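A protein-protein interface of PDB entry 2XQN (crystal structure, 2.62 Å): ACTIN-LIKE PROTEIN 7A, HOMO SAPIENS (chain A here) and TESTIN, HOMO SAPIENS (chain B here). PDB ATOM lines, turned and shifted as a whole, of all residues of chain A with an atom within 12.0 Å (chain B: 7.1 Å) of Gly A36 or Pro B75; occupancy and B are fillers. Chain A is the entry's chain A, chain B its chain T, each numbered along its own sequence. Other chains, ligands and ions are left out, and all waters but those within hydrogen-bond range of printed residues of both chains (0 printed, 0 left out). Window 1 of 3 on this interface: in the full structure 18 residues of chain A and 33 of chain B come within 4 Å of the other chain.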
ATOM      1  N   SER A  32      12.135  -9.530  26.249  1.00  0.00           N
ATOM      2  CA  SER A  32      13.039  -8.634  26.953  1.00  0.00           C
ATOM      3  C   SER A  32      13.952  -7.852  25.966  1.00  0.00           C
ATOM      4  O   SER A  32      14.812  -8.435  25.299  1.00  0.00           O
ATOM      5  CB  SER A  32      13.838  -9.458  27.984  1.00  0.00           C
ATOM      6  OG  SER A  32      14.469  -8.615  28.934  1.00  0.00           O
ATOM      7  N   LEU A  33      13.725  -6.539  25.880  1.00  0.00           N
ATOM      8  CA  LEU A  33      14.496  -5.677  25.035  1.00  0.00           C
ATOM      9  C   LEU A  33      15.897  -5.681  25.559  1.00  0.00           C
ATOM     10  O   LEU A  33      16.109  -5.251  26.660  1.00  0.00           O
ATOM     11  CB  LEU A  33      13.956  -4.249  25.117  1.00  0.00           C
ATOM     12  CG  LEU A  33      12.806  -3.857  24.195  1.00  0.00           C
ATOM     13  CD1 LEU A  33      12.583  -2.340  24.200  1.00  0.00           C
ATOM     14  CD2 LEU A  33      13.083  -4.359  22.769  1.00  0.00           C
ATOM     15  N   ARG A  34      16.851  -6.185  24.789  1.00  0.00           N
ATOM     16  CA  ARG A  34      18.276  -5.999  25.060  1.00  0.00           C
ATOM     17  C   ARG A  34      18.872  -4.795  24.302  1.00  0.00           C
ATOM     18  O   ARG A  34      18.399  -4.410  23.235  1.00  0.00           O
ATOM     19  CB  ARG A  34      19.019  -7.274  24.708  1.00  0.00           C
ATOM     20  CG  ARG A  34      20.506  -7.099  24.320  1.00  0.00           C
ATOM     21  CD  ARG A  34      21.097  -8.412  23.788  1.00  0.00           C
ATOM     22  NE  ARG A  34      20.468  -9.507  24.509  1.00  0.00           N
ATOM     23  CZ  ARG A  34      20.968 -10.071  25.602  1.00  0.00           C
ATOM     24  NH1 ARG A  34      22.142  -9.666  26.073  1.00  0.00           N
ATOM     25  NH2 ARG A  34      20.294 -11.046  26.215  1.00  0.00           N
ATOM     26  N   ASP A  35      19.913  -4.196  24.873  1.00  0.00           N
ATOM     27  CA  ASP A  35      20.581  -3.033  24.274  1.00  0.00           C
ATOM     28  C   ASP A  35      21.484  -3.472  23.145  1.00  0.00           C
ATOM     29  O   ASP A  35      21.978  -4.627  23.164  1.00  0.00           O
ATOM     30  CB  ASP A  35      21.443  -2.358  25.319  1.00  0.00           C
ATOM     31  CG  ASP A  35      20.637  -1.580  26.294  1.00  0.00           C
ATOM     32  OD1 ASP A  35      19.485  -1.232  25.972  1.00  0.00           O
ATOM     33  OD2 ASP A  35      21.158  -1.305  27.381  1.00  0.00           O
ATOM     34  N   GLY A  36      21.688  -2.568  22.177  1.00  0.00           N
ATOM     35  CA  GLY A  36      22.600  -2.817  21.074  1.00  0.00           C
ATOM     36  C   GLY A  36      24.008  -3.048  21.593  1.00  0.00           C
ATOM     37  O   GLY A  36      24.362  -2.535  22.631  1.00  0.00           O
ATOM     38  N   PRO A  37      24.830  -3.827  20.879  1.00  0.00           N
ATOM     39  CA  PRO A  37      26.174  -3.944  21.452  1.00  0.00           C
ATOM     40  C   PRO A  37      27.069  -2.704  21.209  1.00  0.00           C
ATOM     41  O   PRO A  37      28.155  -2.672  21.765  1.00  0.00           O
ATOM     42  CB  PRO A  37      26.755  -5.200  20.769  1.00  0.00           C
ATOM     43  CG  PRO A  37      26.058  -5.244  19.464  1.00  0.00           C
ATOM     44  CD  PRO A  37      24.680  -4.619  19.644  1.00  0.00           C
ATOM     45  N   ALA A  38      26.638  -1.711  20.422  1.00  0.00           N
ATOM     46  CA  ALA A  38      27.479  -0.526  20.174  1.00  0.00           C
ATOM     47  C   ALA A  38      27.776   0.279  21.416  1.00  0.00           C
ATOM     48  O   ALA A  38      26.945   0.381  22.306  1.00  0.00           O
ATOM     49  CB  ALA A  38      26.887   0.374  19.163  1.00  0.00           C
ATOM     50  N   LYS A  39      28.978   0.856  21.452  1.00  0.00           N
ATOM     51  CA  LYS A  39      29.442   1.725  22.529  1.00  0.00           C
ATOM     52  C   LYS A  39      30.157   2.895  21.885  1.00  0.00           C
ATOM     53  O   LYS A  39      30.433   2.872  20.696  1.00  0.00           O
ATOM     54  CB  LYS A  39      30.402   0.942  23.421  1.00  0.00           C
ATOM     55  CG  LYS A  39      29.716  -0.200  24.157  1.00  0.00           C
ATOM     56  CD  LYS A  39      30.499  -0.620  25.372  1.00  0.00           C
ATOM     57  CE  LYS A  39      29.845  -1.856  26.017  1.00  0.00           C
ATOM     58  NZ  LYS A  39      30.938  -2.708  26.630  1.00  0.00           N
ATOM     59  N   ARG A  40      30.425   3.941  22.637  1.00  0.00           N
ATOM     60  CA  ARG A  40      31.235   4.985  22.068  1.00  0.00           C
ATOM     61  C   ARG A  40      32.662   4.957  22.644  1.00  0.00           C
ATOM     62  O   ARG A  40      32.812   4.809  23.858  1.00  0.00           O
ATOM     63  CB  ARG A  40      30.633   6.360  22.268  1.00  0.00           C
ATOM     64  CG  ARG A  40      31.407   7.337  21.420  1.00  0.00           C
ATOM     65  CD  ARG A  40      30.803   8.670  21.406  1.00  0.00           C
ATOM     66  NE  ARG A  40      29.500   8.657  20.762  1.00  0.00           N
ATOM     67  CZ  ARG A  40      29.296   9.004  19.506  1.00  0.00           C
ATOM     68  NH1 ARG A  40      30.310   9.377  18.741  1.00  0.00           N
ATOM     69  NH2 ARG A  40      28.070   8.992  19.041  1.00  0.00           N
ATOM     70  N   ALA A  41      33.691   5.063  21.789  1.00  0.00           N
ATOM     71  CA  ALA A  41      35.075   5.261  22.271  1.00  0.00           C
ATOM     72  C   ALA A  41      35.239   6.739  22.680  1.00  0.00           C
ATOM     73  O   ALA A  41      35.140   7.639  21.829  1.00  0.00           O
ATOM     74  CB  ALA A  41      36.072   4.896  21.212  1.00  0.00           C
ATOM     75  N   ILE B  44      31.687   5.709  17.224  1.00  0.00           N
ATOM     76  CA  ILE B  44      31.002   4.479  17.632  1.00  0.00           C
ATOM     77  C   ILE B  44      31.782   3.237  17.164  1.00  0.00           C
ATOM     78  O   ILE B  44      32.289   3.177  16.017  1.00  0.00           O
ATOM     79  CB  ILE B  44      29.565   4.460  17.078  1.00  0.00           C
ATOM     80  CG1 ILE B  44      28.759   5.703  17.573  1.00  0.00           C
ATOM     81  CG2 ILE B  44      28.900   3.159  17.396  1.00  0.00           C
ATOM     82  CD1 ILE B  44      28.187   5.607  19.041  1.00  0.00           C
ATOM     83  N   TYR B  45      31.866   2.235  18.022  1.00  0.00           N
ATOM     84  CA  TYR B  45      32.467   0.965  17.629  1.00  0.00           C
ATOM     85  C   TYR B  45      31.695  -0.176  18.298  1.00  0.00           C
ATOM     86  O   TYR B  45      30.820   0.083  19.145  1.00  0.00           O
ATOM     87  CB  TYR B  45      33.903   0.908  18.123  1.00  0.00           C
ATOM     88  CG  TYR B  45      33.976   0.710  19.621  1.00  0.00           C
ATOM     89  CD1 TYR B  45      33.944   1.802  20.489  1.00  0.00           C
ATOM     90  CD2 TYR B  45      34.048  -0.571  20.169  1.00  0.00           C
ATOM     91  CE1 TYR B  45      34.002   1.616  21.898  1.00  0.00           C
ATOM     92  CE2 TYR B  45      34.108  -0.781  21.554  1.00  0.00           C
ATOM     93  CZ  TYR B  45      34.087   0.317  22.406  1.00  0.00           C
ATOM     94  OH  TYR B  45      34.159   0.124  23.747  1.00  0.00           O
ATOM     95  N   VAL B  46      32.047  -1.425  17.963  1.00  0.00           N
ATOM     96  CA  VAL B  46      31.377  -2.637  18.519  1.00  0.00           C
ATOM     97  C   VAL B  46      32.428  -3.741  18.810  1.00  0.00           C
ATOM     98  O   VAL B  46      33.376  -3.887  18.062  1.00  0.00           O
ATOM     99  CB  VAL B  46      30.250  -3.195  17.558  1.00  0.00           C
ATOM    100  CG1 VAL B  46      29.375  -4.194  18.272  1.00  0.00           C
ATOM    101  CG2 VAL B  46      29.383  -2.090  17.044  1.00  0.00           C
ATOM    102  N   CYS B  54      34.845  -0.781  13.733  1.00  0.00           N
ATOM    103  CA  CYS B  54      34.125   0.486  13.603  1.00  0.00           C
ATOM    104  C   CYS B  54      32.674   0.249  13.159  1.00  0.00           C
ATOM    105  O   CYS B  54      32.295  -0.879  12.915  1.00  0.00           O
ATOM    106  CB  CYS B  54      34.874   1.499  12.713  1.00  0.00           C
ATOM    107  SG  CYS B  54      34.867   1.154  10.922  1.00  0.00           S
ATOM    108  N   LYS B  55      31.851   1.298  13.099  1.00  0.00           N
ATOM    109  CA  LYS B  55      30.428   1.107  12.770  1.00  0.00           C
ATOM    110  C   LYS B  55      30.271   0.545  11.339  1.00  0.00           C
ATOM    111  O   LYS B  55      29.609  -0.485  11.164  1.00  0.00           O
ATOM    112  CB  LYS B  55      29.618   2.391  13.042  1.00  0.00           C
ATOM    113  CG  LYS B  55      28.234   2.498  12.411  1.00  0.00           C
ATOM    114  CD  LYS B  55      27.208   1.656  13.102  1.00  0.00           C
ATOM    115  CE  LYS B  55      25.792   1.997  12.636  1.00  0.00           C
ATOM    116  NZ  LYS B  55      25.224   3.120  13.412  1.00  0.00           N
ATOM    117  N   TYR B  58      31.290  -3.005  10.978  1.00  0.00           N
ATOM    118  CA  TYR B  58      30.306  -3.892  11.614  1.00  0.00           C
ATOM    119  C   TYR B  58      29.141  -4.134  10.639  1.00  0.00           C
ATOM    120  O   TYR B  58      28.876  -5.283  10.249  1.00  0.00           O
ATOM    121  CB  TYR B  58      29.790  -3.334  12.954  1.00  0.00           C
ATOM    122  CG  TYR B  58      28.754  -4.235  13.626  1.00  0.00           C
ATOM    123  CD1 TYR B  58      29.154  -5.306  14.448  1.00  0.00           C
ATOM    124  CD2 TYR B  58      27.370  -4.031  13.429  1.00  0.00           C
ATOM    125  CE1 TYR B  58      28.212  -6.146  15.052  1.00  0.00           C
ATOM    126  CE2 TYR B  58      26.412  -4.881  14.045  1.00  0.00           C
ATOM    127  CZ  TYR B  58      26.851  -5.936  14.844  1.00  0.00           C
ATOM    128  OH  TYR B  58      25.946  -6.773  15.458  1.00  0.00           O
ATOM    129  N   VAL B  59      28.492  -3.040  10.232  1.00  0.00           N
ATOM    130  CA  VAL B  59      27.406  -3.083   9.276  1.00  0.00           C
ATOM    131  C   VAL B  59      27.805  -3.923   8.047  1.00  0.00           C
ATOM    132  O   VAL B  59      27.035  -4.786   7.625  1.00  0.00           O
ATOM    133  CB  VAL B  59      26.969  -1.659   8.871  1.00  0.00           C
ATOM    134  CG1 VAL B  59      26.354  -1.674   7.528  1.00  0.00           C
ATOM    135  CG2 VAL B  59      25.995  -1.039   9.926  1.00  0.00           C
ATOM    136  N   ALA B  63      27.144  -8.456  10.679  1.00  0.00           N
ATOM    137  CA  ALA B  63      25.831  -9.118  10.655  1.00  0.00           C
ATOM    138  C   ALA B  63      24.971  -8.512  11.691  1.00  0.00           C
ATOM    139  O   ALA B  63      24.957  -7.271  11.783  1.00  0.00           O
ATOM    140  CB  ALA B  63      25.952 -10.696  10.858  1.00  0.00           C
ATOM    141  N   ALA B  72      19.637  -6.261   8.525  1.00  0.00           N
ATOM    142  CA  ALA B  72      20.557  -6.054   9.627  1.00  0.00           C
ATOM    143  C   ALA B  72      19.875  -5.216  10.699  1.00  0.00           C
ATOM    144  O   ALA B  72      19.032  -4.377  10.393  1.00  0.00           O
ATOM    145  CB  ALA B  72      21.840  -5.385   9.147  1.00  0.00           C
ATOM    146  N   ILE B  73      20.216  -5.518  11.945  1.00  0.00           N
ATOM    147  CA  ILE B  73      19.840  -4.736  13.097  1.00  0.00           C
ATOM    148  C   ILE B  73      20.993  -3.834  13.458  1.00  0.00           C
ATOM    149  O   ILE B  73      22.054  -4.318  13.865  1.00  0.00           O
ATOM    150  CB  ILE B  73      19.529  -5.650  14.313  1.00  0.00           C
ATOM    151  CG1 ILE B  73      18.475  -6.696  13.922  1.00  0.00           C
ATOM    152  CG2 ILE B  73      19.115  -4.786  15.523  1.00  0.00           C
ATOM    153  CD1 ILE B  73      17.978  -7.549  15.053  1.00  0.00           C
ATOM    154  N   ASP B  74      20.795  -2.535  13.290  1.00  0.00           N
ATOM    155  CA  ASP B  74      21.737  -1.517  13.750  1.00  0.00           C
ATOM    156  C   ASP B  74      22.306  -1.739  15.195  1.00  0.00           C
ATOM    157  O   ASP B  74      21.555  -1.740  16.199  1.00  0.00           O
ATOM    158  CB  ASP B  74      21.082  -0.119  13.642  1.00  0.00           C
ATOM    159  CG  ASP B  74      22.080   1.036  13.933  1.00  0.00           C
ATOM    160  OD1 ASP B  74      22.837   1.022  14.961  1.00  0.00           O
ATOM    161  OD2 ASP B  74      22.112   1.960  13.105  1.00  0.00           O
ATOM    162  N   PRO B  75      23.640  -1.830  15.320  1.00  0.00           N
ATOM    163  CA  PRO B  75      24.183  -2.109  16.634  1.00  0.00           C
ATOM    164  C   PRO B  75      23.869  -1.024  17.719  1.00  0.00           C
ATOM    165  O   PRO B  75      24.081  -1.296  18.926  1.00  0.00           O
ATOM    166  CB  PRO B  75      25.692  -2.178  16.363  1.00  0.00           C
ATOM    167  CG  PRO B  75      25.924  -1.167  15.289  1.00  0.00           C
ATOM    168  CD  PRO B  75      24.664  -1.250  14.424  1.00  0.00           C
ATOM    169  N   GLU B  76      23.381   0.163  17.319  1.00  0.00           N
ATOM    170  CA  GLU B  76      22.987   1.180  18.322  1.00  0.00           C
ATOM    171  C   GLU B  76      21.611   0.963  18.934  1.00  0.00           C
ATOM    172  O   GLU B  76      21.421   1.249  20.089  1.00  0.00           O
ATOM    173  CB  GLU B  76      23.074   2.581  17.769  1.00  0.00           C
ATOM    174  CG  GLU B  76      24.408   2.817  17.112  1.00  0.00           C
ATOM    175  CD  GLU B  76      24.750   4.269  16.993  1.00  0.00           C
ATOM    176  OE1 GLU B  76      24.998   4.740  15.854  1.00  0.00           O
ATOM    177  OE2 GLU B  76      24.757   4.930  18.061  1.00  0.00           O
ATOM    178  N   VAL B  77      20.663   0.421  18.175  1.00  0.00           N
ATOM    179  CA  VAL B  77      19.272   0.280  18.641  1.00  0.00           C
ATOM    180  C   VAL B  77      19.064  -0.997  19.466  1.00  0.00           C
ATOM    181  O   VAL B  77      19.804  -2.002  19.333  1.00  0.00           O
ATOM    182  CB  VAL B  77      18.254   0.248  17.461  1.00  0.00           C
ATOM    183  CG1 VAL B  77      18.396   1.434  16.552  1.00  0.00           C
ATOM    184  CG2 VAL B  77      18.424  -1.022  16.645  1.00  0.00           C
ATOM    185  N   GLN B  78      18.034  -0.968  20.307  1.00  0.00           N
ATOM    186  CA  GLN B  78      17.648  -2.178  21.047  1.00  0.00           C
ATOM    187  C   GLN B  78      16.968  -3.243  20.142  1.00  0.00           C
ATOM    188  O   GLN B  78      16.409  -2.946  19.082  1.00  0.00           O
ATOM    189  CB  GLN B  78      16.725  -1.813  22.175  1.00  0.00           C
ATOM    190  CG  GLN B  78      17.256  -0.790  23.174  1.00  0.00           C
ATOM    191  CD  GLN B  78      16.205  -0.558  24.278  1.00  0.00           C
ATOM    192  OE1 GLN B  78      15.037  -0.208  23.977  1.00  0.00           O
ATOM    193  NE2 GLN B  78      16.584  -0.836  25.543  1.00  0.00           N
ATOM    194  N   ARG B  79      17.041  -4.496  20.545  1.00  0.00           N
ATOM    195  CA  ARG B  79      16.497  -5.579  19.724  1.00  0.00           C
ATOM    196  C   ARG B  79      16.015  -6.634  20.689  1.00  0.00           C
ATOM    197  O   ARG B  79      16.358  -6.585  21.874  1.00  0.00           O
ATOM    198  CB  ARG B  79      17.555  -6.140  18.750  1.00  0.00           C
ATOM    199  CG  ARG B  79      18.563  -7.133  19.342  1.00  0.00           C
ATOM    200  CD  ARG B  79      19.646  -6.489  20.189  1.00  0.00           C
ATOM    201  NE  ARG B  79      20.118  -5.249  19.583  1.00  0.00           N
ATOM    202  CZ  ARG B  79      20.981  -5.212  18.583  1.00  0.00           C
ATOM    203  NH1 ARG B  79      21.443  -6.351  18.144  1.00  0.00           N
ATOM    204  NH2 ARG B  79      21.377  -4.062  18.034  1.00  0.00           N
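OD1 of Asp A35 sits at hydrogen-bond distance from NE2 of Gln B78, 3.0 Å away.
The backbone NH (N) of Gly A36 sits close to the backbone carbonyl oxygen (O) of Val B77 (3.5 Å).
The backbone NH of Ala A38 lies within hydrogen-bond range of the backbone carbonyl oxygen of Pro B75, 3.0 Å away.
O of Arg B79 sits at hydrogen-bond distance from N of Arg A34 (3.0 Å).
The backbone nitrogen (N) of Pro A37 lies close to the backbone carbonyl oxygen (O) of Pro B75, 3.3 Å away.
The backbone NH of Lys A39 sits at hydrogen-bond distance from the backbone carbonyl oxygen of Tyr B45, at 3.1 Å.
The backbone NH of Glu B76 lies within hydrogen-bond range of the side-chain carboxylate of Asp B74.
The backbone carbonyl oxygen (O) of Ile B44 is in hydrogen-bond range of the backbone NH (N) of Lys B55 (3.5 Å).
The side-chain carboxylate of Glu B76 is in salt-bridge range of the side-chain amino group of Lys B55, at 2.9 Å.
The backbone carbonyl oxygen of Val B77 lies within hydrogen-bond range of the guanidinium group of Arg B79, 2.9 Å away.
O of Asp B74 sits at hydrogen-bond distance from NH2 of Arg B79, at 3.0 Å.
Leu A33 touches Gln B78 (CD1 to OE1, 3.3 Å).
CA of Leu A33 touches O of Arg B79 (3.8 Å).
Gln B78 touches Arg A34 (CA to O, 3.2 Å).
Arg B79 touches Gly A36 (NH2 to CA, 3.5 Å).
Val B46 touches Pro A37.
Ala A38 touches Ile B44 (CB to CG2, 3.9 Å).
Ala A38 touches Val B46.
N of Glu B76 touches CB of Ala A38, 3.97 Å away.
Tyr B45 touches Arg A40.
N of Ala A41 touches CE1 of Tyr B45, at 3.5 Å.
Of chain B, only Pro B75, Val B77 and Arg B79 come within 4 Å of Gly A36.
Of chain A, only Gly A36, Pro A37 and Ala A38 come within 4 Å of Pro B75.
No residue of chain A comes within 4 Å of Lys B55.
Of chain A, only Ala A38 comes within 4 Å of Glu B76.
Of chain A, only Gly A36 comes within 4 Å of Val B77.
Gln B78 touches three residues of chain A.
Of chain A, only Leu A33 (3.8 Å), Arg A34 (3.0 Å), Gly A36 (3.5 Å) and Pro A37 (3.7 Å) come within 4 Å of Arg B79.
Of the printed residues of chain A, Tyr B45 touches Ala A38 (3.5 Å), Lys A39 (3.1 Å), Arg A40 (3.7 Å) and Ala A41 (3.5 Å).
Of the printed residues of chain B, Leu A33 touches Gln B78 (3.3 Å) and Arg B79 (3.8 Å).
Of the printed residues of chain B, Arg A34 touches Gln B78 and Arg B79.
Of the printed residues of chain B, Arg A40 touches Ile B44 and Tyr B45.
Printed residues of chain A within 4 Å of Ile B44: Ala A38, Lys A39 and Arg A40.
Ile B73 touches none of the printed residues of chain A.
The nearest residue of chain B that does not touch Gly A36 is Gln B78 (4.2 Å).
The nearest printed residue of chain B that does not touch Leu A33 is Val B77 (7.6 Å).
Hydrophobic or aromatic side chains of chain A that line the printed part of chain B: Leu A33, Pro A37, Ala A38 and Ala A41.
Printed residues of chain B that touch a printed residue of chain A: Ile B44, Tyr B45, Val B46, Pro B75, Glu B76, Val B77, Gln B78 and Arg B79.
Hydrophobic or aromatic side chains of chain B that line the printed part of chain A: Ile B44, Tyr B45, Val B46 and Pro B75.
Among the printed residues, no Asp or Glu carboxylate lies within 4 Å of a Lys or Arg side-chain nitrogen of the other chain.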
